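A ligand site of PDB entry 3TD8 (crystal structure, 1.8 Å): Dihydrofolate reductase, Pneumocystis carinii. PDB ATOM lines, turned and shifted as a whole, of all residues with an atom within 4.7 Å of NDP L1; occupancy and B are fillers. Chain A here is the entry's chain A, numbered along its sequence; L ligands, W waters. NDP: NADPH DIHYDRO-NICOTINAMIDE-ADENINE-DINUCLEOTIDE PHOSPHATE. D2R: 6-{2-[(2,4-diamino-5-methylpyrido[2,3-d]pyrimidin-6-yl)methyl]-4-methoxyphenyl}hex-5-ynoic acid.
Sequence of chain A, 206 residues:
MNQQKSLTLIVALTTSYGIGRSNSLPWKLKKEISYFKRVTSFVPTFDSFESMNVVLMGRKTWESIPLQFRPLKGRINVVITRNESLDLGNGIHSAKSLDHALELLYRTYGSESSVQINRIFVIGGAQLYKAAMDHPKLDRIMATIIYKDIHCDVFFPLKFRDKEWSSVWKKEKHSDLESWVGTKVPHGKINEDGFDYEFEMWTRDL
The side-chain amide nitrogen (ND2) of Asn 83 is in hydrogen-bond range of the side-chain hydroxyl (OG1) of Thr 81, at 2.8 Å.
N of Gly 125 lies within hydrogen-bond range of OG1 of Thr 61 (2.9 Å).
The backbone NH (N) of Ile 19 lies within hydrogen-bond range of the backbone carbonyl oxygen (O) of Val 154 (3.0 Å).
OG of Ser 64 lies within hydrogen-bond range of O of Lys 60, at 3.1 Å.
The side-chain hydroxyl of Tyr 129 is in hydrogen-bond range of the backbone carbonyl oxygen of Ile 123, at 3.2 Å.
The side-chain hydroxyl (OH) of Tyr 129 sits at hydrogen-bond distance from the backbone carbonyl oxygen (O) of Ile 10, at 2.6 Å.
The backbone carbonyl oxygen of Gly 124 sits at hydrogen-bond distance from the backbone NH of Gly 58.
The side-chain hydroxyl (OG) of Ser 64 sits at hydrogen-bond distance from the backbone carbonyl oxygen (O) of Asn 23 (2.7 Å).
The backbone carbonyl oxygen (O) of Ile 80 sits close to an oxygen (O4B) of NDP L1 (3.4 Å).
Val 11 touches NDP L1 (CA to O7N, 3.5 Å).
Gly 20 touches NDP L1 (CA to O3D, 3.3 Å).
Arg 21 touches NDP L1 (N to O3D, 3.8 Å).
Asn 23 touches NDP L1 (C to O2D, 3.7 Å).
CD1 of Leu 25 touches C2N of NDP L1, at 3.5 Å.
Trp 27 touches NDP L1.
CA of Gly 58 touches O1A of NDP L1, 3.5 Å away.
Asn 83 touches NDP L1.
Lys 96 touches NDP L1 (O to C2A, 3.3 Å).
Ile 123 touches NDP L1 (O to C4N, 3.2 Å).
CA of Gly 124 touches C5N of NDP L1, at 3.8 Å.
Tyr 129 touches NDP L1 (OH to C4N, 3.4 Å).
CB of Ala 131 touches N6A of NDP L1, 3.3 Å away.
Val 154 touches NDP L1.
Water W1 bridges the side-chain amide nitrogen (ND2) of Asn 83 (2.9 Å) and an oxygen (O2X) of NDP L1 (3.1 Å).
Water W2 bridges N of Asn 23 and O3D of NDP L1.
O2D of NDP L1 lies close to OAT of D2R L2, at 3.1 Å.
N of Ala 12 is in hydrogen-bond range of O7N of NDP L1.
O of Ala 12 sits at hydrogen-bond distance from N7N of NDP L1, 2.6 Å away.
An oxygen (O2X) of NDP L1 is in hydrogen-bond range of the side-chain hydroxyl (OG1) of Thr 81, 2.6 Å away.
The backbone NH (N) of Arg 59 lies within hydrogen-bond range of an oxygen (O4B) of NDP L1 (3.1 Å).
An oxygen (O2X) of NDP L1 lies within salt-bridge range of the guanidinium group of Arg 59 (2.6 Å).
O1A of NDP L1 is in hydrogen-bond range of N of Thr 61 (2.8 Å).
An oxygen (O1A) of NDP L1 lies within hydrogen-bond range of the side-chain hydroxyl of Thr 61.
The backbone NH of Arg 82 is in hydrogen-bond range of an oxygen (O1X) of NDP L1 (2.7 Å).
N of Gln 127 sits at hydrogen-bond distance from O1N of NDP L1.
O1A of NDP L1 sits at hydrogen-bond distance from N of Gly 125.
O of Ile 19 lies within hydrogen-bond range of N7N of NDP L1, 3.0 Å away.
An oxygen (O2D) of NDP L1 sits close to the backbone NH (N) of Ser 24 (3.5 Å).
An oxygen (O2D) of NDP L1 sits at hydrogen-bond distance from the backbone carbonyl oxygen (O) of Ser 24, at 3.1 Å.
The backbone NH (N) of Ala 126 lies within hydrogen-bond range of an oxygen (O5D) of NDP L1 (3.1 Å).
N of Lys 60 lies within hydrogen-bond range of O5B of NDP L1, 3.2 Å away.
The backbone NH (N) of Leu 128 is in hydrogen-bond range of an oxygen (O2A) of NDP L1 (3.3 Å).
The backbone carbonyl oxygen (O) of Ile 123 sits at hydrogen-bond distance from a nitrogen (NAD) of D2R L2 (2.8 Å).
A nitrogen (NAD) of D2R L2 lies within hydrogen-bond range of the side-chain hydroxyl (OH) of Tyr 129 (3.5 Å).
The backbone carbonyl oxygen (O) of Val 11 lies close to a nitrogen (NAC) of D2R L2 (3.4 Å).
NAD of D2R L2 lies within hydrogen-bond range of O of Ile 10 (3.0 Å).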
ATOM      1  N   ILE A  10     -26.877 -15.566  14.007  1.00  0.00           N
ATOM      2  CA  ILE A  10     -27.022 -16.881  14.714  1.00  0.00           C
ATOM      3  C   ILE A  10     -25.972 -16.938  15.892  1.00  0.00           C
ATOM      4  O   ILE A  10     -24.797 -16.570  15.767  1.00  0.00           O
ATOM      5  CB  ILE A  10     -26.883 -18.074  13.723  1.00  0.00           C
ATOM      6  CG1 ILE A  10     -27.125 -19.442  14.451  1.00  0.00           C
ATOM      7  CG2 ILE A  10     -25.567 -18.004  12.906  1.00  0.00           C
ATOM      8  CD1 ILE A  10     -27.374 -20.645  13.457  1.00  0.00           C
ATOM      9  N   VAL A  11     -26.481 -17.356  17.056  1.00  0.00           N
ATOM     10  CA  VAL A  11     -25.794 -17.292  18.317  1.00  0.00           C
ATOM     11  C   VAL A  11     -26.395 -18.355  19.281  1.00  0.00           C
ATOM     12  O   VAL A  11     -27.599 -18.689  19.219  1.00  0.00           O
ATOM     13  CB  VAL A  11     -25.972 -15.871  18.957  1.00  0.00           C
ATOM     14  CG1 VAL A  11     -27.443 -15.496  19.253  1.00  0.00           C
ATOM     15  CG2 VAL A  11     -25.086 -15.641  20.191  1.00  0.00           C
ATOM     16  N   ALA A  12     -25.598 -18.788  20.251  1.00  0.00           N
ATOM     17  CA  ALA A  12     -26.082 -19.622  21.322  1.00  0.00           C
ATOM     18  C   ALA A  12     -25.649 -18.810  22.532  1.00  0.00           C
ATOM     19  O   ALA A  12     -24.505 -18.330  22.576  1.00  0.00           O
ATOM     20  CB  ALA A  12     -25.392 -21.024  21.324  1.00  0.00           C
ATOM     21  N   ILE A  19     -22.087 -15.650  25.919  1.00  0.00           N
ATOM     22  CA  ILE A  19     -21.795 -16.341  24.671  1.00  0.00           C
ATOM     23  C   ILE A  19     -20.423 -17.014  24.608  1.00  0.00           C
ATOM     24  O   ILE A  19     -20.173 -17.774  23.692  1.00  0.00           O
ATOM     25  CB  ILE A  19     -22.060 -15.477  23.392  1.00  0.00           C
ATOM     26  CG1 ILE A  19     -20.994 -14.375  23.240  1.00  0.00           C
ATOM     27  CG2 ILE A  19     -23.514 -14.980  23.460  1.00  0.00           C
ATOM     28  CD1 ILE A  19     -21.100 -13.394  22.088  1.00  0.00           C
ATOM     29  N   GLY A  20     -19.560 -16.721  25.575  1.00  0.00           N
ATOM     30  CA  GLY A  20     -18.135 -17.029  25.416  1.00  0.00           C
ATOM     31  C   GLY A  20     -17.320 -17.044  26.681  1.00  0.00           C
ATOM     32  O   GLY A  20     -17.664 -16.393  27.677  1.00  0.00           O
ATOM     33  N   ARG A  21     -16.206 -17.775  26.662  1.00  0.00           N
ATOM     34  CA  ARG A  21     -15.364 -17.862  27.863  1.00  0.00           C
ATOM     35  C   ARG A  21     -14.001 -18.251  27.363  1.00  0.00           C
ATOM     36  O   ARG A  21     -13.890 -19.280  26.677  1.00  0.00           O
ATOM     37  CB  ARG A  21     -15.911 -18.915  28.845  1.00  0.00           C
ATOM     38  CG  ARG A  21     -15.433 -18.640  30.259  1.00  0.00           C
ATOM     39  CD  ARG A  21     -15.312 -19.858  31.164  1.00  0.00           C
ATOM     40  NE  ARG A  21     -14.792 -19.465  32.485  1.00  0.00           N
ATOM     41  CZ  ARG A  21     -14.007 -18.390  32.761  1.00  0.00           C
ATOM     42  NH1 ARG A  21     -13.616 -18.180  34.009  1.00  0.00           N
ATOM     43  NH2 ARG A  21     -13.603 -17.533  31.821  1.00  0.00           N
ATOM     44  N   ASN A  23     -11.892 -17.246  24.975  1.00  0.00           N
ATOM     45  CA  ASN A  23     -11.908 -17.389  23.481  1.00  0.00           C
ATOM     46  C   ASN A  23     -12.481 -18.675  22.913  1.00  0.00           C
ATOM     47  O   ASN A  23     -12.058 -19.155  21.847  1.00  0.00           O
ATOM     48  CB  ASN A  23     -10.527 -17.143  22.903  1.00  0.00           C
ATOM     49  CG  ASN A  23     -10.025 -15.767  23.245  1.00  0.00           C
ATOM     50  OD1 ASN A  23     -10.774 -14.798  23.184  1.00  0.00           O
ATOM     51  ND2 ASN A  23      -8.760 -15.676  23.622  1.00  0.00           N
ATOM     52  N   SER A  24     -13.417 -19.259  23.640  1.00  0.00           N
ATOM     53  CA  SER A  24     -14.127 -20.443  23.155  1.00  0.00           C
ATOM     54  C   SER A  24     -15.566 -20.398  23.670  1.00  0.00           C
ATOM     55  O   SER A  24     -15.939 -19.430  24.371  1.00  0.00           O
ATOM     56  CB  SER A  24     -13.437 -21.726  23.645  1.00  0.00           C
ATOM     57  OG  SER A  24     -13.798 -22.850  22.829  1.00  0.00           O
ATOM     58  N   LEU A  25     -16.347 -21.417  23.327  1.00  0.00           N
ATOM     59  CA  LEU A  25     -17.679 -21.667  23.892  1.00  0.00           C
ATOM     60  C   LEU A  25     -17.523 -22.393  25.216  1.00  0.00           C
ATOM     61  O   LEU A  25     -16.812 -23.402  25.293  1.00  0.00           O
ATOM     62  CB  LEU A  25     -18.534 -22.519  22.931  1.00  0.00           C
ATOM     63  CG  LEU A  25     -19.129 -22.013  21.604  1.00  0.00           C
ATOM     64  CD1 LEU A  25     -18.920 -20.538  21.300  1.00  0.00           C
ATOM     65  CD2 LEU A  25     -18.828 -22.918  20.429  1.00  0.00           C
ATOM     66  N   TRP A  27     -19.462 -24.477  26.549  1.00  0.00           N
ATOM     67  CA  TRP A  27     -20.259 -25.694  26.504  1.00  0.00           C
ATOM     68  C   TRP A  27     -19.831 -26.469  25.316  1.00  0.00           C
ATOM     69  O   TRP A  27     -19.283 -25.912  24.341  1.00  0.00           O
ATOM     70  CB  TRP A  27     -21.785 -25.412  26.463  1.00  0.00           C
ATOM     71  CG  TRP A  27     -22.120 -24.306  25.490  1.00  0.00           C
ATOM     72  CD1 TRP A  27     -22.208 -24.380  24.101  1.00  0.00           C
ATOM     73  CD2 TRP A  27     -22.348 -22.880  25.808  1.00  0.00           C
ATOM     74  NE1 TRP A  27     -22.477 -23.143  23.568  1.00  0.00           N
ATOM     75  CE2 TRP A  27     -22.560 -22.197  24.524  1.00  0.00           C
ATOM     76  CE3 TRP A  27     -22.406 -22.133  26.991  1.00  0.00           C
ATOM     77  CZ2 TRP A  27     -22.818 -20.813  24.440  1.00  0.00           C
ATOM     78  CZ3 TRP A  27     -22.664 -20.749  26.908  1.00  0.00           C
ATOM     79  CH2 TRP A  27     -22.877 -20.114  25.657  1.00  0.00           C
ATOM     80  N   GLY A  58     -16.190 -12.181  13.122  1.00  0.00           N
ATOM     81  CA  GLY A  58     -15.085 -11.362  13.572  1.00  0.00           C
ATOM     82  C   GLY A  58     -13.751 -12.122  13.507  1.00  0.00           C
ATOM     83  O   GLY A  58     -13.730 -13.369  13.481  1.00  0.00           O
ATOM     84  N   ARG A  59     -12.653 -11.374  13.532  1.00  0.00           N
ATOM     85  CA  ARG A  59     -11.324 -12.030  13.514  1.00  0.00           C
ATOM     86  C   ARG A  59     -11.145 -12.905  14.749  1.00  0.00           C
ATOM     87  O   ARG A  59     -10.604 -13.992  14.629  1.00  0.00           O
ATOM     88  CB  ARG A  59     -10.182 -11.031  13.359  1.00  0.00           C
ATOM     89  CG  ARG A  59      -8.807 -11.702  13.478  1.00  0.00           C
ATOM     90  CD  ARG A  59      -7.702 -10.661  13.388  1.00  0.00           C
ATOM     91  NE  ARG A  59      -7.850  -9.623  14.431  1.00  0.00           N
ATOM     92  CZ  ARG A  59      -7.541  -9.794  15.723  1.00  0.00           C
ATOM     93  NH1 ARG A  59      -7.054 -10.945  16.157  1.00  0.00           N
ATOM     94  NH2 ARG A  59      -7.689  -8.810  16.593  1.00  0.00           N
ATOM     95  N   LYS A  60     -11.609 -12.472  15.918  1.00  0.00           N
ATOM     96  CA  LYS A  60     -11.418 -13.285  17.145  1.00  0.00           C
ATOM     97  C   LYS A  60     -12.124 -14.644  17.079  1.00  0.00           C
ATOM     98  O   LYS A  60     -11.524 -15.648  17.389  1.00  0.00           O
ATOM     99  CB  LYS A  60     -11.715 -12.512  18.449  1.00  0.00           C
ATOM    100  CG  LYS A  60     -10.748 -11.345  18.573  1.00  0.00           C
ATOM    101  CD  LYS A  60     -10.945 -10.401  19.745  1.00  0.00           C
ATOM    102  CE  LYS A  60      -9.736 -10.476  20.674  1.00  0.00           C
ATOM    103  NZ  LYS A  60      -9.628  -9.224  21.484  1.00  0.00           N
ATOM    104  N   THR A  61     -13.377 -14.646  16.619  1.00  0.00           N
ATOM    105  CA  THR A  61     -14.135 -15.854  16.324  1.00  0.00           C
ATOM    106  C   THR A  61     -13.397 -16.733  15.282  1.00  0.00           C
ATOM    107  O   THR A  61     -13.306 -17.957  15.443  1.00  0.00           O
ATOM    108  CB  THR A  61     -15.551 -15.459  15.844  1.00  0.00           C
ATOM    109  OG1 THR A  61     -16.218 -14.847  16.976  1.00  0.00           O
ATOM    110  CG2 THR A  61     -16.305 -16.629  15.236  1.00  0.00           C
ATOM    111  N   SER A  64     -10.684 -18.549  17.028  1.00  0.00           N
ATOM    112  CA  SER A  64     -11.270 -19.496  18.017  1.00  0.00           C
ATOM    113  C   SER A  64     -11.729 -20.835  17.431  1.00  0.00           C
ATOM    114  O   SER A  64     -11.786 -21.829  18.131  1.00  0.00           O
ATOM    115  CB  SER A  64     -12.476 -18.871  18.708  1.00  0.00           C
ATOM    116  OG  SER A  64     -12.092 -17.788  19.513  1.00  0.00           O
ATOM    117  N   ILE A  80     -14.209 -10.324   9.101  1.00  0.00           N
ATOM    118  CA  ILE A  80     -14.201  -8.856   9.278  1.00  0.00           C
ATOM    119  C   ILE A  80     -13.047  -8.383  10.188  1.00  0.00           C
ATOM    120  O   ILE A  80     -12.880  -8.834  11.335  1.00  0.00           O
ATOM    121  CB  ILE A  80     -15.554  -8.305   9.829  1.00  0.00           C
ATOM    122  CG1 ILE A  80     -16.785  -8.882   9.063  1.00  0.00           C
ATOM    123  CG2 ILE A  80     -15.549  -6.768   9.833  1.00  0.00           C
ATOM    124  CD1 ILE A  80     -16.617  -8.989   7.579  1.00  0.00           C
ATOM    125  N   THR A  81     -12.199  -7.520   9.654  1.00  0.00           N
ATOM    126  CA  THR A  81     -11.052  -7.007  10.436  1.00  0.00           C
ATOM    127  C   THR A  81     -10.690  -5.636   9.857  1.00  0.00           C
ATOM    128  O   THR A  81     -10.725  -5.439   8.658  1.00  0.00           O
ATOM    129  CB  THR A  81      -9.804  -7.960  10.408  1.00  0.00           C
ATOM    130  OG1 THR A  81      -8.626  -7.160  10.619  1.00  0.00           O
ATOM    131  CG2 THR A  81      -9.650  -8.661   9.050  1.00  0.00           C
ATOM    132  N   ARG A  82     -10.370  -4.715  10.732  1.00  0.00           N
ATOM    133  CA  ARG A  82     -10.066  -3.389  10.346  1.00  0.00           C
ATOM    134  C   ARG A  82      -8.679  -3.360   9.811  1.00  0.00           C
ATOM    135  O   ARG A  82      -8.164  -2.328   9.507  1.00  0.00           O
ATOM    136  CB  ARG A  82     -10.236  -2.458  11.513  1.00  0.00           C
ATOM    137  CG  ARG A  82     -11.675  -2.130  11.816  1.00  0.00           C
ATOM    138  CD  ARG A  82     -11.836  -1.500  13.174  1.00  0.00           C
ATOM    139  NE  ARG A  82     -13.116  -0.865  13.306  1.00  0.00           N
ATOM    140  CZ  ARG A  82     -14.064  -1.309  14.104  1.00  0.00           C
ATOM    141  NH1 ARG A  82     -13.848  -2.394  14.818  1.00  0.00           N
ATOM    142  NH2 ARG A  82     -15.217  -0.689  14.181  1.00  0.00           N
ATOM    143  N   ASN A  83      -8.057  -4.488   9.636  1.00  0.00           N
ATOM    144  CA  ASN A  83      -6.771  -4.334   9.061  1.00  0.00           C
ATOM    145  C   ASN A  83      -6.356  -5.284   8.024  1.00  0.00           C
ATOM    146  O   ASN A  83      -6.189  -6.456   8.226  1.00  0.00           O
ATOM    147  CB  ASN A  83      -5.718  -4.140  10.129  1.00  0.00           C
ATOM    148  CG  ASN A  83      -5.114  -5.421  10.564  1.00  0.00           C
ATOM    149  OD1 ASN A  83      -3.921  -5.530  10.770  1.00  0.00           O
ATOM    150  ND2 ASN A  83      -5.943  -6.403  10.688  1.00  0.00           N
ATOM    151  N   LYS A  96     -13.390  -4.945   5.768  1.00  0.00           N
ATOM    152  CA  LYS A  96     -13.085  -4.052   6.873  1.00  0.00           C
ATOM    153  C   LYS A  96     -14.333  -3.653   7.632  1.00  0.00           C
ATOM    154  O   LYS A  96     -14.225  -3.048   8.662  1.00  0.00           O
ATOM    155  CB  LYS A  96     -12.218  -2.840   6.433  1.00  0.00           C
ATOM    156  CG  LYS A  96     -12.869  -1.879   5.461  1.00  0.00           C
ATOM    157  CD  LYS A  96     -11.807  -0.902   4.893  1.00  0.00           C
ATOM    158  CE  LYS A  96     -12.203  -0.494   3.470  1.00  0.00           C
ATOM    159  NZ  LYS A  96     -11.212   0.378   2.768  1.00  0.00           N
ATOM    160  N   SER A  97     -15.516  -4.025   7.121  1.00  0.00           N
ATOM    161  CA  SER A  97     -16.720  -3.828   7.880  1.00  0.00           C
ATOM    162  C   SER A  97     -17.791  -4.704   7.296  1.00  0.00           C
ATOM    163  O   SER A  97     -17.559  -5.317   6.241  1.00  0.00           O
ATOM    164  CB  SER A  97     -17.206  -2.372   7.751  1.00  0.00           C
ATOM    165  OG  SER A  97     -17.599  -2.093   6.392  1.00  0.00           O
ATOM    166  N   ILE A 123     -21.996 -14.669  12.417  1.00  0.00           N
ATOM    167  CA  ILE A 123     -21.888 -15.863  13.314  1.00  0.00           C
ATOM    168  C   ILE A 123     -21.072 -15.539  14.542  1.00  0.00           C
ATOM    169  O   ILE A 123     -20.793 -16.439  15.314  1.00  0.00           O
ATOM    170  CB  ILE A 123     -21.278 -17.072  12.581  1.00  0.00           C
ATOM    171  CG1 ILE A 123     -19.803 -16.784  12.133  1.00  0.00           C
ATOM    172  CG2 ILE A 123     -22.212 -17.446  11.421  1.00  0.00           C
ATOM    173  CD1 ILE A 123     -18.999 -18.075  11.842  1.00  0.00           C
ATOM    174  N   GLY A 124     -20.666 -14.283  14.690  1.00  0.00           N
ATOM    175  CA  GLY A 124     -20.014 -13.840  15.942  1.00  0.00           C
ATOM    176  C   GLY A 124     -18.722 -13.148  15.640  1.00  0.00           C
ATOM    177  O   GLY A 124     -18.395 -13.014  14.465  1.00  0.00           O
ATOM    178  N   GLY A 125     -18.000 -12.610  16.651  1.00  0.00           N
ATOM    179  CA  GLY A 125     -18.377 -12.649  18.079  1.00  0.00           C
ATOM    180  C   GLY A 125     -19.175 -11.436  18.534  1.00  0.00           C
ATOM    181  O   GLY A 125     -19.867 -10.793  17.762  1.00  0.00           O
ATOM    182  N   ALA A 126     -19.010 -11.077  19.799  1.00  0.00           N
ATOM    183  CA  ALA A 126     -19.785  -9.934  20.367  1.00  0.00           C
ATOM    184  C   ALA A 126     -19.621  -8.663  19.567  1.00  0.00           C
ATOM    185  O   ALA A 126     -20.582  -7.977  19.368  1.00  0.00           O
ATOM    186  CB  ALA A 126     -19.372  -9.649  21.821  1.00  0.00           C
ATOM    187  N   GLN A 127     -18.416  -8.293  19.184  1.00  0.00           N
ATOM    188  CA  GLN A 127     -18.191  -7.042  18.481  1.00  0.00           C
ATOM    189  C   GLN A 127     -18.903  -6.996  17.110  1.00  0.00           C
ATOM    190  O   GLN A 127     -19.587  -5.979  16.747  1.00  0.00           O
ATOM    191  CB  GLN A 127     -16.685  -6.845  18.331  1.00  0.00           C
ATOM    192  CG  GLN A 127     -16.337  -5.519  17.684  1.00  0.00           C
ATOM    193  CD  GLN A 127     -14.875  -5.133  17.918  1.00  0.00           C
ATOM    194  OE1 GLN A 127     -14.330  -4.336  17.161  1.00  0.00           O
ATOM    195  NE2 GLN A 127     -14.264  -5.649  19.000  1.00  0.00           N
ATOM    196  N   LEU A 128     -18.764  -8.075  16.351  1.00  0.00           N
ATOM    197  CA  LEU A 128     -19.521  -8.216  15.101  1.00  0.00           C
ATOM    198  C   LEU A 128     -21.021  -8.305  15.321  1.00  0.00           C
ATOM    199  O   LEU A 128     -21.756  -7.714  14.534  1.00  0.00           O
ATOM    200  CB  LEU A 128     -19.024  -9.395  14.256  1.00  0.00           C
ATOM    201  CG  LEU A 128     -18.875  -9.237  12.750  1.00  0.00           C
ATOM    202  CD1 LEU A 128     -19.128 -10.523  11.948  1.00  0.00           C
ATOM    203  CD2 LEU A 128     -19.640  -8.076  12.159  1.00  0.00           C
ATOM    204  N   TYR A 129     -21.476  -8.962  16.371  1.00  0.00           N
ATOM    205  CA  TYR A 129     -22.835  -8.988  16.736  1.00  0.00           C
ATOM    206  C   TYR A 129     -23.371  -7.561  16.950  1.00  0.00           C
ATOM    207  O   TYR A 129     -24.480  -7.210  16.491  1.00  0.00           O
ATOM    208  CB  TYR A 129     -23.099  -9.798  18.036  1.00  0.00           C
ATOM    209  CG  TYR A 129     -23.081 -11.313  17.823  1.00  0.00           C
ATOM    210  CD1 TYR A 129     -23.557 -11.888  16.645  1.00  0.00           C
ATOM    211  CD2 TYR A 129     -22.595 -12.152  18.806  1.00  0.00           C
ATOM    212  CE1 TYR A 129     -23.589 -13.275  16.445  1.00  0.00           C
ATOM    213  CE2 TYR A 129     -22.595 -13.500  18.598  1.00  0.00           C
ATOM    214  CZ  TYR A 129     -23.043 -14.068  17.418  1.00  0.00           C
ATOM    215  OH  TYR A 129     -23.001 -15.460  17.341  1.00  0.00           O
ATOM    216  N   ALA A 131     -22.287  -4.766  15.763  1.00  0.00           N
ATOM    217  CA  ALA A 131     -22.371  -4.042  14.496  1.00  0.00           C
ATOM    218  C   ALA A 131     -23.568  -4.535  13.703  1.00  0.00           C
ATOM    219  O   ALA A 131     -24.258  -3.705  13.069  1.00  0.00           O
ATOM    220  CB  ALA A 131     -21.133  -4.263  13.685  1.00  0.00           C
ATOM    221  N   VAL A 154     -17.676 -13.059  27.784  1.00  0.00           N
ATOM    222  CA  VAL A 154     -18.104 -12.261  26.624  1.00  0.00           C
ATOM    223  C   VAL A 154     -19.589 -12.489  26.532  1.00  0.00           C
ATOM    224  O   VAL A 154     -20.087 -13.609  26.711  1.00  0.00           O
ATOM    225  CB  VAL A 154     -17.524 -12.816  25.289  1.00  0.00           C
ATOM    226  CG1 VAL A 154     -18.122 -12.042  24.106  1.00  0.00           C
ATOM    227  CG2 VAL A 154     -15.999 -12.717  25.193  1.00  0.00           C
HETATM  228  PA  NDP L   1     -15.110 -11.009  17.407  1.00  0.00           P
HETATM  229  O1A NDP L   1     -15.084 -12.396  16.894  1.00  0.00           O
HETATM  230  O2A NDP L   1     -16.222 -10.030  17.097  1.00  0.00           O
HETATM  231  O5B NDP L   1     -13.789 -10.350  16.816  1.00  0.00           O
HETATM  232  C5B NDP L   1     -13.423  -8.977  17.113  1.00  0.00           C
HETATM  233  C4B NDP L   1     -12.556  -8.424  16.058  1.00  0.00           C
HETATM  234  O4B NDP L   1     -13.150  -8.584  14.705  1.00  0.00           O
HETATM  235  C3B NDP L   1     -12.282  -6.974  16.201  1.00  0.00           C
HETATM  236  O3B NDP L   1     -11.073  -6.730  16.949  1.00  0.00           O
HETATM  237  C2B NDP L   1     -12.004  -6.631  14.716  1.00  0.00           C
HETATM  238  O2B NDP L   1     -10.779  -7.212  14.238  1.00  0.00           O
HETATM  239  C1B NDP L   1     -13.104  -7.390  13.995  1.00  0.00           C
HETATM  240  N9A NDP L   1     -14.427  -6.734  14.056  1.00  0.00           N
HETATM  241  C8A NDP L   1     -15.515  -7.089  14.766  1.00  0.00           C
HETATM  242  N7A NDP L   1     -16.545  -6.212  14.496  1.00  0.00           N
HETATM  243  C5A NDP L   1     -16.072  -5.350  13.587  1.00  0.00           C
HETATM  244  C6A NDP L   1     -16.645  -4.264  12.935  1.00  0.00           C
HETATM  245  N6A NDP L   1     -17.929  -3.892  13.188  1.00  0.00           N
HETATM  246  N1A NDP L   1     -15.861  -3.612  12.044  1.00  0.00           N
HETATM  247  C2A NDP L   1     -14.586  -3.956  11.813  1.00  0.00           C
HETATM  248  N3A NDP L   1     -14.000  -4.992  12.417  1.00  0.00           N
HETATM  249  C4A NDP L   1     -14.719  -5.668  13.332  1.00  0.00           C
HETATM  250  O3  NDP L   1     -14.764 -11.027  18.964  1.00  0.00           O
HETATM  251  PN  NDP L   1     -15.382 -10.767  20.301  1.00  0.00           P
HETATM  252  O1N NDP L   1     -16.191  -9.521  20.378  1.00  0.00           O
HETATM  253  O2N NDP L   1     -14.246 -10.842  21.274  1.00  0.00           O
HETATM  254  O5D NDP L   1     -16.150 -12.094  20.548  1.00  0.00           O
HETATM  255  C5D NDP L   1     -15.400 -13.398  20.493  1.00  0.00           C
HETATM  256  C4D NDP L   1     -15.998 -14.266  21.598  1.00  0.00           C
HETATM  257  O4D NDP L   1     -17.329 -14.608  21.088  1.00  0.00           O
HETATM  258  C3D NDP L   1     -15.398 -15.614  22.061  1.00  0.00           C
HETATM  259  O3D NDP L   1     -15.810 -15.867  23.450  1.00  0.00           O
HETATM  260  C2D NDP L   1     -16.084 -16.587  21.170  1.00  0.00           C
HETATM  261  O2D NDP L   1     -15.946 -17.920  21.702  1.00  0.00           O
HETATM  262  C1D NDP L   1     -17.524 -16.059  21.367  1.00  0.00           C
HETATM  263  N1N NDP L   1     -18.500 -16.518  20.382  1.00  0.00           N
HETATM  264  C2N NDP L   1     -19.707 -17.128  20.774  1.00  0.00           C
HETATM  265  C3N NDP L   1     -20.649 -17.542  19.847  1.00  0.00           C
HETATM  266  C7N NDP L   1     -21.962 -18.175  20.268  1.00  0.00           C
HETATM  267  O7N NDP L   1     -22.781 -18.528  19.457  1.00  0.00           O
HETATM  268  N7N NDP L   1     -22.143 -18.449  21.568  1.00  0.00           N
HETATM  269  C4N NDP L   1     -20.381 -17.337  18.338  1.00  0.00           C
HETATM  270  C5N NDP L   1     -19.110 -16.813  18.063  1.00  0.00           C
HETATM  271  C6N NDP L   1     -18.210 -16.370  19.025  1.00  0.00           C
HETATM  272  P2B NDP L   1      -9.382  -6.356  14.064  1.00  0.00           P
HETATM  273  O1X NDP L   1      -9.605  -5.077  13.317  1.00  0.00           O
HETATM  274  O2X NDP L   1      -8.569  -7.403  13.179  1.00  0.00           O
HETATM  275  O3X NDP L   1      -9.028  -6.294  15.625  1.00  0.00           O
HETATM  276  N1  D2R L   2     -24.123 -19.932  16.748  1.00  0.00           N
HETATM  277  C2  D2R L   2     -24.535 -21.055  17.355  1.00  0.00           C
HETATM  278  N3  D2R L   2     -23.700 -22.067  17.608  1.00  0.00           N
HETATM  279  C4  D2R L   2     -22.435 -21.988  17.200  1.00  0.00           C
HETATM  280  C5  D2R L   2     -21.910 -20.807  16.587  1.00  0.00           C
HETATM  281  C6  D2R L   2     -22.851 -19.722  16.399  1.00  0.00           C
HETATM  282  CAA D2R L   2     -15.511 -19.172  19.027  1.00  0.00           C
HETATM  283  CAB D2R L   2     -19.807 -19.601  15.489  1.00  0.00           C
HETATM  284  NAC D2R L   2     -25.825 -21.196  17.736  1.00  0.00           N
HETATM  285  NAD D2R L   2     -22.509 -18.558  15.832  1.00  0.00           N
HETATM  286  OAE D2R L   2     -20.097 -25.518  11.320  1.00  0.00           O
HETATM  287  OAF D2R L   2     -18.876 -26.881  10.081  1.00  0.00           O
HETATM  288  CAG D2R L   2     -17.249 -25.448  15.615  1.00  0.00           C
HETATM  289  CAH D2R L   2     -16.948 -24.550  16.371  1.00  0.00           C
HETATM  290  CAI D2R L   2     -15.363 -22.666  19.188  1.00  0.00           C
HETATM  291  CAJ D2R L   2     -15.681 -23.711  18.313  1.00  0.00           C
HETATM  292  CAK D2R L   2     -20.363 -23.002  17.051  1.00  0.00           C
HETATM  293  CAL D2R L   2     -16.909 -21.200  17.960  1.00  0.00           C
HETATM  294  CAM D2R L   2     -17.550 -26.596  14.728  1.00  0.00           C
HETATM  295  CAN D2R L   2     -18.526 -26.111  13.672  1.00  0.00           C
HETATM  296  CAO D2R L   2     -18.402 -26.905  12.382  1.00  0.00           C
HETATM  297  CAP D2R L   2     -18.236 -21.999  16.013  1.00  0.00           C
HETATM  298  NAQ D2R L   2     -21.651 -23.051  17.432  1.00  0.00           N
HETATM  299  OAT D2R L   2     -15.682 -20.358  19.819  1.00  0.00           O
HETATM  300  CAU D2R L   2     -19.186 -26.381  11.176  1.00  0.00           C
HETATM  301  CAX D2R L   2     -20.543 -20.782  16.177  1.00  0.00           C
HETATM  302  CAY D2R L   2     -15.972 -21.406  18.991  1.00  0.00           C
HETATM  303  CAZ D2R L   2     -16.610 -23.494  17.276  1.00  0.00           C
HETATM  304  CBA D2R L   2     -19.748 -21.914  16.435  1.00  0.00           C
HETATM  305  CBB D2R L   2     -17.252 -22.248  17.115  1.00  0.00           C
HETATM  306  O   HOH W   1      -5.530  -6.995  13.542  1.00  0.00           O
HETATM  307  O   HOH W   2     -13.675 -15.242  25.610  1.00  0.00           O
HETATM  308  O   HOH W   3     -19.277  -3.249  10.377  1.00  0.00           O
